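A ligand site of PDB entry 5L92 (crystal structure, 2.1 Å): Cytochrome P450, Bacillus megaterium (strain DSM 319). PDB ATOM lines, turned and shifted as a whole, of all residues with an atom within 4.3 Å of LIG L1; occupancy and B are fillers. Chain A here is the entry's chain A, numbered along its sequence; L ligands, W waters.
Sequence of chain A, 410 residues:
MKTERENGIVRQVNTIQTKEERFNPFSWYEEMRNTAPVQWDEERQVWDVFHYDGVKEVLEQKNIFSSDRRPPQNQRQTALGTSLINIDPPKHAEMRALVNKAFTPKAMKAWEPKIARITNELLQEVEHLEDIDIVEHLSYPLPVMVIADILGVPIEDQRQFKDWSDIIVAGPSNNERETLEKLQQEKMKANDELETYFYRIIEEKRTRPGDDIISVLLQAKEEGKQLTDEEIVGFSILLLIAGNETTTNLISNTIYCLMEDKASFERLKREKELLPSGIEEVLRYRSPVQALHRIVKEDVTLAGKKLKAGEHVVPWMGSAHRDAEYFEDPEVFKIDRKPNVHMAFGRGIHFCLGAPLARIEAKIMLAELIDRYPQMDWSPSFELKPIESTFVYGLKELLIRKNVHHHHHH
SG of Cys 352 binds FE1 of LIG L1 (2.4 Å).
An oxygen (O4) of LIG L1 lies within hydrogen-bond range of a ring nitrogen (ND1) of His 350 (2.7 Å).
NE2 of His 92 sits at hydrogen-bond distance from O3 of LIG L1, 2.6 Å away.
The guanidinium group (NH2) of Arg 96 is in salt-bridge range of an oxygen (O3) of LIG L1 (2.9 Å).
The guanidinium group of Arg 294 is in salt-bridge range of an oxygen (O1) of LIG L1 (2.9 Å).
An oxygen (O1) of LG2 L2 is bound to an iron atom (FE1) of LIG L1.
The backbone carbonyl oxygen of Ile 349 sits close to a ring nitrogen (NE2) of His 92, 3.5 Å away.
A ring nitrogen (ND1) of His 350 sits close to the backbone carbonyl oxygen of Leu 84, 3.4 Å away.
N of Cys 352 is in hydrogen-bond range of O of Phe 345 (2.9 Å).
The backbone carbonyl oxygen (O) of Ile 349 is in hydrogen-bond range of the guanidinium group (NH2) of Arg 96, at 3.3 Å.
The side-chain sulfur of Cys 352 lies close to the backbone NH of Gly 354 (3.1 Å).
A ring nitrogen (NE2) of His 92 is in hydrogen-bond range of a ring nitrogen (ND1) of His 350.
The side-chain hydroxyl (OG1) of Thr 246 lies within hydrogen-bond range of the backbone carbonyl oxygen (O) of Ala 242 (2.8 Å).
The backbone carbonyl oxygen (O) of Ile 85 is in hydrogen-bond range of the guanidinium group (NH1) of Arg 69 (3.3 Å).
The backbone carbonyl oxygen (O) of Leu 84 sits close to an oxygen (O4) of LIG L1 (3.1 Å).
Merely in contact with LIG L1: Thr 246 (3.1 Å), Ile 85 (3.4 Å), Phe 345 (3.4 Å), Leu 239 (3.4 Å), Ala 344 (3.4 Å), Gly 346 (3.4 Å), Gly 354 (3.5 Å), Leu 292 (3.6 Å), Leu 250 (3.6 Å), Ala 242 (3.6 Å), Ile 349 (3.6 Å), Leu 238 (3.6 Å), Thr 247 (3.6 Å), Ala 358 (3.6 Å), Leu 353 (3.7 Å), Pro 288 (3.8 Å), Met 317 (3.8 Å), Phe 103 (3.96 Å) and Val 289 (3.97 Å).
Water W3 lies within hydrogen-bond range of O of Ile 85 (2.7 Å), O2 of LIG L1 (2.8 Å), NH2 of Arg 69 (3.2 Å) and NH1 of Arg 294 (3.3 Å).
Water W1 lies within hydrogen-bond range of the backbone carbonyl oxygen of Ala 242 (2.9 Å), the side-chain hydroxyl of Thr 247 (3.1 Å) and the side-chain hydroxyl of Thr 246 (3.4 Å).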
ATOM      1  N   ARG A  69      14.635 -10.038  31.180  1.00  0.00           N
ATOM      2  CA  ARG A  69      14.916 -11.218  30.410  1.00  0.00           C
ATOM      3  C   ARG A  69      16.154 -10.947  29.576  1.00  0.00           C
ATOM      4  O   ARG A  69      16.145 -10.172  28.646  1.00  0.00           O
ATOM      5  CB  ARG A  69      13.719 -11.610  29.552  1.00  0.00           C
ATOM      6  CG  ARG A  69      12.366 -11.081  29.989  1.00  0.00           C
ATOM      7  CD  ARG A  69      11.354 -12.187  30.231  1.00  0.00           C
ATOM      8  NE  ARG A  69      10.474 -11.938  31.367  1.00  0.00           N
ATOM      9  CZ  ARG A  69       9.531 -11.022  31.386  1.00  0.00           C
ATOM     10  NH1 ARG A  69       9.323 -10.256  30.361  1.00  0.00           N
ATOM     11  NH2 ARG A  69       8.806 -10.875  32.429  1.00  0.00           N
ATOM     12  N   LEU A  84       8.846  -1.483  29.064  1.00  0.00           N
ATOM     13  CA  LEU A  84       8.153  -1.658  30.326  1.00  0.00           C
ATOM     14  C   LEU A  84       8.024  -3.101  30.771  1.00  0.00           C
ATOM     15  O   LEU A  84       8.255  -3.395  31.948  1.00  0.00           O
ATOM     16  CB  LEU A  84       6.734  -1.096  30.245  1.00  0.00           C
ATOM     17  CG  LEU A  84       6.558   0.396  30.358  1.00  0.00           C
ATOM     18  CD1 LEU A  84       5.077   0.649  30.162  1.00  0.00           C
ATOM     19  CD2 LEU A  84       7.015   0.921  31.689  1.00  0.00           C
ATOM     20  N   ILE A  85       7.642  -3.987  29.864  1.00  0.00           N
ATOM     21  CA  ILE A  85       7.364  -5.371  30.262  1.00  0.00           C
ATOM     22  C   ILE A  85       8.603  -6.137  30.666  1.00  0.00           C
ATOM     23  O   ILE A  85       8.472  -7.187  31.323  1.00  0.00           O
ATOM     24  CB  ILE A  85       6.608  -6.109  29.125  1.00  0.00           C
ATOM     25  CG1 ILE A  85       5.963  -7.387  29.665  1.00  0.00           C
ATOM     26  CG2 ILE A  85       7.525  -6.419  27.947  1.00  0.00           C
ATOM     27  CD1 ILE A  85       4.809  -7.920  28.817  1.00  0.00           C
ATOM     28  N   HIS A  92      11.573   0.813  36.055  1.00  0.00           N
ATOM     29  CA  HIS A  92      10.202   0.533  35.593  1.00  0.00           C
ATOM     30  C   HIS A  92       9.268   1.673  35.954  1.00  0.00           C
ATOM     31  O   HIS A  92       8.474   2.116  35.127  1.00  0.00           O
ATOM     32  CB  HIS A  92       9.655  -0.764  36.190  1.00  0.00           C
ATOM     33  CG  HIS A  92       8.215  -0.979  35.834  1.00  0.00           C
ATOM     34  ND1 HIS A  92       7.181  -0.582  36.654  1.00  0.00           N
ATOM     35  CD2 HIS A  92       7.642  -1.474  34.703  1.00  0.00           C
ATOM     36  CE1 HIS A  92       6.020  -0.868  36.067  1.00  0.00           C
ATOM     37  NE2 HIS A  92       6.272  -1.409  34.884  1.00  0.00           N
ATOM     38  N   ARG A  96       7.032   3.856  33.279  1.00  0.00           N
ATOM     39  CA  ARG A  96       5.583   3.761  33.345  1.00  0.00           C
ATOM     40  C   ARG A  96       4.975   5.109  33.686  1.00  0.00           C
ATOM     41  O   ARG A  96       3.882   5.460  33.215  1.00  0.00           O
ATOM     42  CB  ARG A  96       5.216   2.679  34.373  1.00  0.00           C
ATOM     43  CG  ARG A  96       3.815   2.705  34.890  1.00  0.00           C
ATOM     44  CD  ARG A  96       2.828   2.134  33.898  1.00  0.00           C
ATOM     45  NE  ARG A  96       2.728   0.688  34.013  1.00  0.00           N
ATOM     46  CZ  ARG A  96       1.604  -0.014  34.171  1.00  0.00           C
ATOM     47  NH1 ARG A  96       0.428   0.568  34.301  1.00  0.00           N
ATOM     48  NH2 ARG A  96       1.680  -1.344  34.234  1.00  0.00           N
ATOM     49  N   PHE A 103      -3.375   6.299  29.483  1.00  0.00           N
ATOM     50  CA  PHE A 103      -4.123   5.043  29.364  1.00  0.00           C
ATOM     51  C   PHE A 103      -5.077   4.760  30.532  1.00  0.00           C
ATOM     52  O   PHE A 103      -5.489   3.608  30.709  1.00  0.00           O
ATOM     53  CB  PHE A 103      -3.175   3.844  29.200  1.00  0.00           C
ATOM     54  CG  PHE A 103      -2.557   3.792  27.849  1.00  0.00           C
ATOM     55  CD1 PHE A 103      -3.283   3.358  26.772  1.00  0.00           C
ATOM     56  CD2 PHE A 103      -1.266   4.227  27.659  1.00  0.00           C
ATOM     57  CE1 PHE A 103      -2.709   3.350  25.517  1.00  0.00           C
ATOM     58  CE2 PHE A 103      -0.710   4.215  26.434  1.00  0.00           C
ATOM     59  CZ  PHE A 103      -1.413   3.787  25.358  1.00  0.00           C
ATOM     60  N   ILE A 147      -5.033   0.748  17.752  1.00  0.00           N
ATOM     61  CA  ILE A 147      -3.634   0.913  18.151  1.00  0.00           C
ATOM     62  C   ILE A 147      -2.835   1.686  17.110  1.00  0.00           C
ATOM     63  O   ILE A 147      -1.915   2.421  17.454  1.00  0.00           O
ATOM     64  CB  ILE A 147      -2.960  -0.459  18.447  1.00  0.00           C
ATOM     65  CG1 ILE A 147      -1.794  -0.291  19.414  1.00  0.00           C
ATOM     66  CG2 ILE A 147      -2.409  -1.101  17.150  1.00  0.00           C
ATOM     67  CD1 ILE A 147      -2.196   0.127  20.813  1.00  0.00           C
ATOM     68  N   LEU A 238       5.948  -2.800  21.643  1.00  0.00           N
ATOM     69  CA  LEU A 238       5.123  -3.520  22.614  1.00  0.00           C
ATOM     70  C   LEU A 238       3.651  -3.226  22.388  1.00  0.00           C
ATOM     71  O   LEU A 238       2.831  -4.145  22.355  1.00  0.00           O
ATOM     72  CB  LEU A 238       5.538  -3.106  24.024  1.00  0.00           C
ATOM     73  CG  LEU A 238       4.777  -3.676  25.229  1.00  0.00           C
ATOM     74  CD1 LEU A 238       4.822  -5.225  25.265  1.00  0.00           C
ATOM     75  CD2 LEU A 238       5.381  -3.077  26.477  1.00  0.00           C
ATOM     76  N   LEU A 239       3.309  -1.953  22.169  1.00  0.00           N
ATOM     77  CA  LEU A 239       1.906  -1.584  21.970  1.00  0.00           C
ATOM     78  C   LEU A 239       1.408  -2.148  20.656  1.00  0.00           C
ATOM     79  O   LEU A 239       0.285  -2.655  20.580  1.00  0.00           O
ATOM     80  CB  LEU A 239       1.710  -0.068  21.980  1.00  0.00           C
ATOM     81  CG  LEU A 239       1.922   0.724  23.253  1.00  0.00           C
ATOM     82  CD1 LEU A 239       1.417   2.159  22.960  1.00  0.00           C
ATOM     83  CD2 LEU A 239       1.252   0.154  24.431  1.00  0.00           C
ATOM     84  N   ALA A 242       0.724  -5.796  21.170  1.00  0.00           N
ATOM     85  CA  ALA A 242      -0.475  -5.793  21.984  1.00  0.00           C
ATOM     86  C   ALA A 242      -1.718  -5.468  21.166  1.00  0.00           C
ATOM     87  O   ALA A 242      -2.779  -6.055  21.361  1.00  0.00           O
ATOM     88  CB  ALA A 242      -0.338  -4.785  23.103  1.00  0.00           C
ATOM     89  N   THR A 246      -3.899  -9.486  21.592  1.00  0.00           N
ATOM     90  CA  THR A 246      -4.531  -9.663  22.904  1.00  0.00           C
ATOM     91  C   THR A 246      -6.039  -9.501  22.840  1.00  0.00           C
ATOM     92  O   THR A 246      -6.774 -10.495  22.880  1.00  0.00           O
ATOM     93  CB  THR A 246      -3.954  -8.678  23.905  1.00  0.00           C
ATOM     94  OG1 THR A 246      -4.173  -7.349  23.428  1.00  0.00           O
ATOM     95  CG2 THR A 246      -2.462  -8.896  24.107  1.00  0.00           C
ATOM     96  N   THR A 247      -6.539  -8.251  22.732  1.00  0.00           N
ATOM     97  CA  THR A 247      -7.964  -7.984  22.714  1.00  0.00           C
ATOM     98  C   THR A 247      -8.697  -8.798  21.667  1.00  0.00           C
ATOM     99  O   THR A 247      -9.847  -9.207  21.884  1.00  0.00           O
ATOM    100  CB  THR A 247      -8.215  -6.486  22.490  1.00  0.00           C
ATOM    101  OG1 THR A 247      -7.613  -5.759  23.553  1.00  0.00           O
ATOM    102  CG2 THR A 247      -9.692  -6.164  22.443  1.00  0.00           C
ATOM    103  N   LEU A 250      -9.692 -11.832  23.443  1.00  0.00           N
ATOM    104  CA  LEU A 250     -10.745 -11.650  24.421  1.00  0.00           C
ATOM    105  C   LEU A 250     -12.114 -11.697  23.732  1.00  0.00           C
ATOM    106  O   LEU A 250     -13.032 -12.381  24.203  1.00  0.00           O
ATOM    107  CB  LEU A 250     -10.551 -10.318  25.150  1.00  0.00           C
ATOM    108  CG  LEU A 250     -11.609  -9.907  26.183  1.00  0.00           C
ATOM    109  CD1 LEU A 250     -11.861 -11.007  27.230  1.00  0.00           C
ATOM    110  CD2 LEU A 250     -11.172  -8.585  26.867  1.00  0.00           C
ATOM    111  N   LEU A 283     -12.275 -13.450  30.708  1.00  0.00           N
ATOM    112  CA  LEU A 283     -10.901 -13.217  31.144  1.00  0.00           C
ATOM    113  C   LEU A 283     -10.443 -14.263  32.153  1.00  0.00           C
ATOM    114  O   LEU A 283      -9.242 -14.564  32.226  1.00  0.00           O
ATOM    115  CB  LEU A 283     -10.778 -11.823  31.778  1.00  0.00           C
ATOM    116  CG  LEU A 283     -10.821 -10.720  30.738  1.00  0.00           C
ATOM    117  CD1 LEU A 283     -11.147  -9.371  31.365  1.00  0.00           C
ATOM    118  CD2 LEU A 283      -9.477 -10.658  29.968  1.00  0.00           C
ATOM    119  N   PRO A 288      -6.870 -14.741  27.487  1.00  0.00           N
ATOM    120  CA  PRO A 288      -5.967 -14.495  26.337  1.00  0.00           C
ATOM    121  C   PRO A 288      -4.493 -14.743  26.612  1.00  0.00           C
ATOM    122  O   PRO A 288      -3.742 -15.076  25.691  1.00  0.00           O
ATOM    123  CB  PRO A 288      -6.232 -13.004  26.042  1.00  0.00           C
ATOM    124  CG  PRO A 288      -7.664 -12.812  26.513  1.00  0.00           C
ATOM    125  CD  PRO A 288      -7.693 -13.554  27.787  1.00  0.00           C
ATOM    126  N   VAL A 289      -4.061 -14.565  27.865  1.00  0.00           N
ATOM    127  CA  VAL A 289      -2.699 -14.876  28.287  1.00  0.00           C
ATOM    128  C   VAL A 289      -2.787 -15.927  29.400  1.00  0.00           C
ATOM    129  O   VAL A 289      -3.344 -15.661  30.469  1.00  0.00           O
ATOM    130  CB  VAL A 289      -1.942 -13.634  28.743  1.00  0.00           C
ATOM    131  CG1 VAL A 289      -0.500 -13.989  29.159  1.00  0.00           C
ATOM    132  CG2 VAL A 289      -1.894 -12.555  27.597  1.00  0.00           C
ATOM    133  N   LEU A 292       2.912 -16.333  32.317  1.00  0.00           N
ATOM    134  CA  LEU A 292       3.968 -15.355  32.135  1.00  0.00           C
ATOM    135  C   LEU A 292       5.297 -16.016  32.494  1.00  0.00           C
ATOM    136  O   LEU A 292       5.348 -17.220  32.814  1.00  0.00           O
ATOM    137  CB  LEU A 292       3.680 -14.116  33.006  1.00  0.00           C
ATOM    138  CG  LEU A 292       2.383 -13.408  32.620  1.00  0.00           C
ATOM    139  CD1 LEU A 292       1.994 -12.324  33.615  1.00  0.00           C
ATOM    140  CD2 LEU A 292       2.579 -12.796  31.249  1.00  0.00           C
ATOM    141  N   ARG A 294       9.137 -15.319  34.673  1.00  0.00           N
ATOM    142  CA  ARG A 294       9.978 -14.568  35.591  1.00  0.00           C
ATOM    143  C   ARG A 294      11.292 -15.311  35.764  1.00  0.00           C
ATOM    144  O   ARG A 294      11.408 -16.505  35.437  1.00  0.00           O
ATOM    145  CB  ARG A 294       9.307 -14.350  36.957  1.00  0.00           C
ATOM    146  CG  ARG A 294       7.961 -13.523  36.950  1.00  0.00           C
ATOM    147  CD  ARG A 294       8.245 -12.108  36.594  1.00  0.00           C
ATOM    148  NE  ARG A 294       7.147 -11.140  36.793  1.00  0.00           N
ATOM    149  CZ  ARG A 294       6.304 -10.754  35.846  1.00  0.00           C
ATOM    150  NH1 ARG A 294       6.318 -11.291  34.629  1.00  0.00           N
ATOM    151  NH2 ARG A 294       5.392  -9.853  36.140  1.00  0.00           N
ATOM    152  N   MET A 317      -1.533 -18.074  35.098  1.00  0.00           N
ATOM    153  CA  MET A 317      -2.782 -17.421  35.489  1.00  0.00           C
ATOM    154  C   MET A 317      -3.991 -18.266  35.082  1.00  0.00           C
ATOM    155  O   MET A 317      -4.969 -18.334  35.827  1.00  0.00           O
ATOM    156  CB  MET A 317      -2.879 -16.016  34.901  1.00  0.00           C
ATOM    157  CG  MET A 317      -1.790 -15.087  35.453  1.00  0.00           C
ATOM    158  SD  MET A 317      -0.412 -15.019  34.303  1.00  0.00           S
ATOM    159  CE  MET A 317      -1.197 -13.944  33.121  1.00  0.00           C
ATOM    160  N   ALA A 344      -5.983 -11.912  34.853  1.00  0.00           N
ATOM    161  CA  ALA A 344      -5.768 -12.063  33.425  1.00  0.00           C
ATOM    162  C   ALA A 344      -4.952 -10.904  32.860  1.00  0.00           C
ATOM    163  O   ALA A 344      -4.357 -11.051  31.800  1.00  0.00           O
ATOM    164  CB  ALA A 344      -7.117 -12.205  32.712  1.00  0.00           C
ATOM    165  N   PHE A 345      -4.889  -9.784  33.577  1.00  0.00           N
ATOM    166  CA  PHE A 345      -4.048  -8.658  33.220  1.00  0.00           C
ATOM    167  C   PHE A 345      -2.766  -8.625  34.051  1.00  0.00           C
ATOM    168  O   PHE A 345      -2.086  -7.601  34.071  1.00  0.00           O
ATOM    169  CB  PHE A 345      -4.809  -7.345  33.407  1.00  0.00           C
ATOM    170  CG  PHE A 345      -5.940  -7.168  32.448  1.00  0.00           C
ATOM    171  CD1 PHE A 345      -5.704  -7.085  31.099  1.00  0.00           C
ATOM    172  CD2 PHE A 345      -7.255  -7.102  32.902  1.00  0.00           C
ATOM    173  CE1 PHE A 345      -6.743  -6.925  30.221  1.00  0.00           C
ATOM    174  CE2 PHE A 345      -8.300  -6.916  32.004  1.00  0.00           C
ATOM    175  CZ  PHE A 345      -8.041  -6.841  30.674  1.00  0.00           C
ATOM    176  N   GLY A 346      -2.455  -9.703  34.748  1.00  0.00           N
ATOM    177  CA  GLY A 346      -1.335  -9.687  35.655  1.00  0.00           C
ATOM    178  C   GLY A 346      -1.741  -9.154  37.009  1.00  0.00           C
ATOM    179  O   GLY A 346      -2.899  -9.153  37.377  1.00  0.00           O
ATOM    180  N   ILE A 349       3.230  -4.367  39.772  1.00  0.00           N
ATOM    181  CA  ILE A 349       3.680  -3.175  39.045  1.00  0.00           C
ATOM    182  C   ILE A 349       3.585  -3.325  37.538  1.00  0.00           C
ATOM    183  O   ILE A 349       3.529  -2.308  36.837  1.00  0.00           O
ATOM    184  CB  ILE A 349       5.118  -2.811  39.432  1.00  0.00           C
ATOM    185  CG1 ILE A 349       6.097  -3.870  38.880  1.00  0.00           C
ATOM    186  CG2 ILE A 349       5.220  -2.734  40.932  1.00  0.00           C
ATOM    187  CD1 ILE A 349       7.509  -3.444  38.926  1.00  0.00           C
ATOM    188  N   HIS A 350       3.532  -4.538  36.989  1.00  0.00           N
ATOM    189  CA  HIS A 350       3.433  -4.703  35.545  1.00  0.00           C
ATOM    190  C   HIS A 350       2.010  -4.933  35.067  1.00  0.00           C
ATOM    191  O   HIS A 350       1.816  -5.236  33.884  1.00  0.00           O
ATOM    192  CB  HIS A 350       4.315  -5.870  35.053  1.00  0.00           C
ATOM    193  CG  HIS A 350       5.773  -5.656  35.271  1.00  0.00           C
ATOM    194  ND1 HIS A 350       6.537  -4.824  34.485  1.00  0.00           N
ATOM    195  CD2 HIS A 350       6.608  -6.189  36.190  1.00  0.00           C
ATOM    196  CE1 HIS A 350       7.787  -4.848  34.913  1.00  0.00           C
ATOM    197  NE2 HIS A 350       7.853  -5.668  35.946  1.00  0.00           N
ATOM    198  N   PHE A 351       1.025  -4.755  35.950  1.00  0.00           N
ATOM    199  CA  PHE A 351      -0.381  -4.891  35.586  1.00  0.00           C
ATOM    200  C   PHE A 351      -0.674  -4.173  34.269  1.00  0.00           C
ATOM    201  O   PHE A 351      -0.321  -3.007  34.093  1.00  0.00           O
ATOM    202  CB  PHE A 351      -1.272  -4.324  36.698  1.00  0.00           C
ATOM    203  CG  PHE A 351      -2.754  -4.491  36.446  1.00  0.00           C
ATOM    204  CD1 PHE A 351      -3.423  -5.610  36.929  1.00  0.00           C
ATOM    205  CD2 PHE A 351      -3.471  -3.529  35.757  1.00  0.00           C
ATOM    206  CE1 PHE A 351      -4.798  -5.783  36.694  1.00  0.00           C
ATOM    207  CE2 PHE A 351      -4.841  -3.667  35.551  1.00  0.00           C
ATOM    208  CZ  PHE A 351      -5.509  -4.800  36.005  1.00  0.00           C
ATOM    209  N   CYS A 352      -1.392  -4.851  33.376  1.00  0.00           N
ATOM    210  CA  CYS A 352      -1.507  -4.417  31.999  1.00  0.00           C
ATOM    211  C   CYS A 352      -1.905  -2.936  31.881  1.00  0.00           C
ATOM    212  O   CYS A 352      -2.956  -2.513  32.361  1.00  0.00           O
ATOM    213  CB  CYS A 352      -2.546  -5.272  31.291  1.00  0.00           C
ATOM    214  SG  CYS A 352      -2.955  -4.742  29.683  1.00  0.00           S
ATOM    215  N   LEU A 353      -1.052  -2.178  31.199  1.00  0.00           N
ATOM    216  CA  LEU A 353      -1.352  -0.783  30.874  1.00  0.00           C
ATOM    217  C   LEU A 353      -2.621  -0.665  30.034  1.00  0.00           C
ATOM    218  O   LEU A 353      -3.336   0.332  30.122  1.00  0.00           O
ATOM    219  CB  LEU A 353      -0.156  -0.191  30.080  1.00  0.00           C
ATOM    220  CG  LEU A 353      -0.242   1.278  29.631  1.00  0.00           C
ATOM    221  CD1 LEU A 353      -0.298   2.160  30.845  1.00  0.00           C
ATOM    222  CD2 LEU A 353       0.957   1.662  28.731  1.00  0.00           C
ATOM    223  N   GLY A 354      -2.880  -1.652  29.165  1.00  0.00           N
ATOM    224  CA  GLY A 354      -3.965  -1.542  28.231  1.00  0.00           C
ATOM    225  C   GLY A 354      -5.297  -2.072  28.727  1.00  0.00           C
ATOM    226  O   GLY A 354      -6.266  -2.117  27.954  1.00  0.00           O
ATOM    227  N   LEU A 357      -8.500   0.044  27.895  1.00  0.00           N
ATOM    228  CA  LEU A 357      -8.766  -0.018  26.469  1.00  0.00           C
ATOM    229  C   LEU A 357      -9.314  -1.365  26.061  1.00  0.00           C
ATOM    230  O   LEU A 357     -10.288  -1.442  25.314  1.00  0.00           O
ATOM    231  CB  LEU A 357      -7.498   0.317  25.691  1.00  0.00           C
ATOM    232  CG  LEU A 357      -7.623   0.247  24.172  1.00  0.00           C
ATOM    233  CD1 LEU A 357      -8.638   1.264  23.692  1.00  0.00           C
ATOM    234  CD2 LEU A 357      -6.276   0.475  23.492  1.00  0.00           C
ATOM    235  N   ALA A 358      -8.693  -2.459  26.541  1.00  0.00           N
ATOM    236  CA  ALA A 358      -9.168  -3.788  26.160  1.00  0.00           C
ATOM    237  C   ALA A 358     -10.627  -3.999  26.577  1.00  0.00           C
ATOM    238  O   ALA A 358     -11.462  -4.418  25.770  1.00  0.00           O
ATOM    239  CB  ALA A 358      -8.253  -4.862  26.781  1.00  0.00           C
HETATM  240  C1  LIG L   1       1.167  -6.013  30.391  1.00  0.00           C
HETATM  241  C2  LIG L   1      -2.531  -9.039  29.333  1.00  0.00           C
HETATM  242  C3  LIG L   1      -4.320  -5.875  26.182  1.00  0.00           C
HETATM  243  C4  LIG L   1      -0.390  -3.144  26.889  1.00  0.00           C
HETATM  244  C5  LIG L   1       0.276  -7.084  30.407  1.00  0.00           C
HETATM  245  C6  LIG L   1       0.340  -8.213  31.306  1.00  0.00           C
HETATM  246  C7  LIG L   1      -0.667  -9.044  31.003  1.00  0.00           C
HETATM  247  C8  LIG L   1      -1.421  -8.465  29.910  1.00  0.00           C
HETATM  248  C9  LIG L   1      -0.985 -10.379  31.706  1.00  0.00           C
HETATM  249  C10 LIG L   1       1.400  -8.429  32.413  1.00  0.00           C
HETATM  250  C11 LIG L   1       2.801  -8.701  31.849  1.00  0.00           C
HETATM  251  C12 LIG L   1       3.737  -9.247  32.888  1.00  0.00           C
HETATM  252  O1  LIG L   1       3.478  -9.121  34.094  1.00  0.00           O
HETATM  253  O2  LIG L   1       4.781  -9.826  32.528  1.00  0.00           O
HETATM  254  C13 LIG L   1      -3.381  -8.455  28.421  1.00  0.00           C
HETATM  255  C14 LIG L   1      -4.684  -8.940  27.988  1.00  0.00           C
HETATM  256  C15 LIG L   1      -5.149  -8.051  27.099  1.00  0.00           C
HETATM  257  C16 LIG L   1      -4.171  -6.998  26.943  1.00  0.00           C
HETATM  258  C17 LIG L   1      -5.366 -10.220  28.505  1.00  0.00           C
HETATM  259  C18 LIG L   1      -6.503  -8.012  26.338  1.00  0.00           C
HETATM  260  C19 LIG L   1      -7.603  -8.646  26.775  1.00  0.00           C
HETATM  261  C20 LIG L   1      -3.412  -4.849  26.101  1.00  0.00           C
HETATM  262  C21 LIG L   1      -3.479  -3.729  25.206  1.00  0.00           C
HETATM  263  C22 LIG L   1      -2.417  -2.977  25.413  1.00  0.00           C
HETATM  264  C23 LIG L   1      -1.596  -3.603  26.417  1.00  0.00           C
HETATM  265  C24 LIG L   1      -4.615  -3.403  24.200  1.00  0.00           C
HETATM  266  C25 LIG L   1      -2.143  -1.700  24.613  1.00  0.00           C
HETATM  267  C26 LIG L   1      -2.009  -0.539  25.237  1.00  0.00           C
HETATM  268  C27 LIG L   1       0.376  -3.668  27.891  1.00  0.00           C
HETATM  269  C28 LIG L   1       1.625  -3.106  28.365  1.00  0.00           C
HETATM  270  C29 LIG L   1       2.075  -3.891  29.350  1.00  0.00           C
HETATM  271  C30 LIG L   1       1.116  -4.982  29.505  1.00  0.00           C
HETATM  272  C31 LIG L   1       2.249  -1.823  27.751  1.00  0.00           C
HETATM  273  C32 LIG L   1       3.365  -3.739  30.198  1.00  0.00           C
HETATM  274  C33 LIG L   1       3.076  -2.973  31.504  1.00  0.00           C
HETATM  275  C34 LIG L   1       4.267  -2.921  32.454  1.00  0.00           C
HETATM  276  O3  LIG L   1       4.304  -2.037  33.328  1.00  0.00           O
HETATM  277  O4  LIG L   1       5.188  -3.771  32.371  1.00  0.00           O
HETATM  278  N1  LIG L   1      -0.815  -7.246  29.561  1.00  0.00           N
HETATM  279  N2  LIG L   1      -3.099  -7.288  27.752  1.00  0.00           N
HETATM  280  N3  LIG L   1      -2.234  -4.752  26.826  1.00  0.00           N
HETATM  281  N4  LIG L   1       0.125  -4.818  28.589  1.00  0.00           N
HETATM  282 FE1  LIG L   1      -1.570  -5.951  28.215  1.00  0.00          FE
HETATM  283  C1  LG2 L   2       1.752  -9.765  26.669  1.00  0.00           C
HETATM  284  C2  LG2 L   2       0.446  -9.062  27.067  1.00  0.00           C
HETATM  285  C3  LG2 L   2       0.231  -7.604  26.436  1.00  0.00           C
HETATM  286  C4  LG2 L   2       0.986  -7.298  25.048  1.00  0.00           C
HETATM  287  C5  LG2 L   2       1.992  -8.320  24.518  1.00  0.00           C
HETATM  288  C6  LG2 L   2       2.691  -8.058  23.131  1.00  0.00           C
HETATM  289  C7  LG2 L   2       4.297  -8.292  23.284  1.00  0.00           C
HETATM  290  C8  LG2 L   2       4.612  -9.636  23.918  1.00  0.00           C
HETATM  291  C9  LG2 L   2       3.848  -9.892  25.289  1.00  0.00           C
HETATM  292  C10 LG2 L   2       2.301  -9.648  25.282  1.00  0.00           C
HETATM  293  C11 LG2 L   2       4.334 -11.308  25.880  1.00  0.00           C
HETATM  294  C12 LG2 L   2       5.971 -11.404  25.958  1.00  0.00           C
HETATM  295  C13 LG2 L   2       6.675 -11.165  24.644  1.00  0.00           C
HETATM  296  C14 LG2 L   2       6.145  -9.739  24.029  1.00  0.00           C
HETATM  297  C15 LG2 L   2       6.806  -9.627  22.879  1.00  0.00           C
HETATM  298  C16 LG2 L   2       8.283 -10.184  23.243  1.00  0.00           C
HETATM  299  C17 LG2 L   2       8.007 -10.949  24.731  1.00  0.00           C
HETATM  300  C18 LG2 L   2       6.380 -12.338  23.648  1.00  0.00           C
HETATM  301  C19 LG2 L   2       1.562 -10.681  24.414  1.00  0.00           C
HETATM  302  C20 LG2 L   2       8.919 -12.199  24.899  1.00  0.00           C
HETATM  303  C21 LG2 L   2       9.634 -12.515  26.223  1.00  0.00           C
HETATM  304  O1  LG2 L   2      -0.532  -6.734  26.856  1.00  0.00           O
HETATM  305  O2  LG2 L   2       3.861 -12.307  25.144  1.00  0.00           O
HETATM  306  O3  LG2 L   2       9.090 -12.953  23.946  1.00  0.00           O
HETATM  307  O4  LG2 L   2      10.216 -13.811  26.080  1.00  0.00           O
HETATM  308  O   HOH W   1      -5.550  -5.119  21.309  1.00  0.00           O
HETATM  309  O   HOH W   2       1.837  -8.372  36.165  1.00  0.00           O
HETATM  310  O   HOH W   3       7.033  -8.323  33.273  1.00  0.00           O
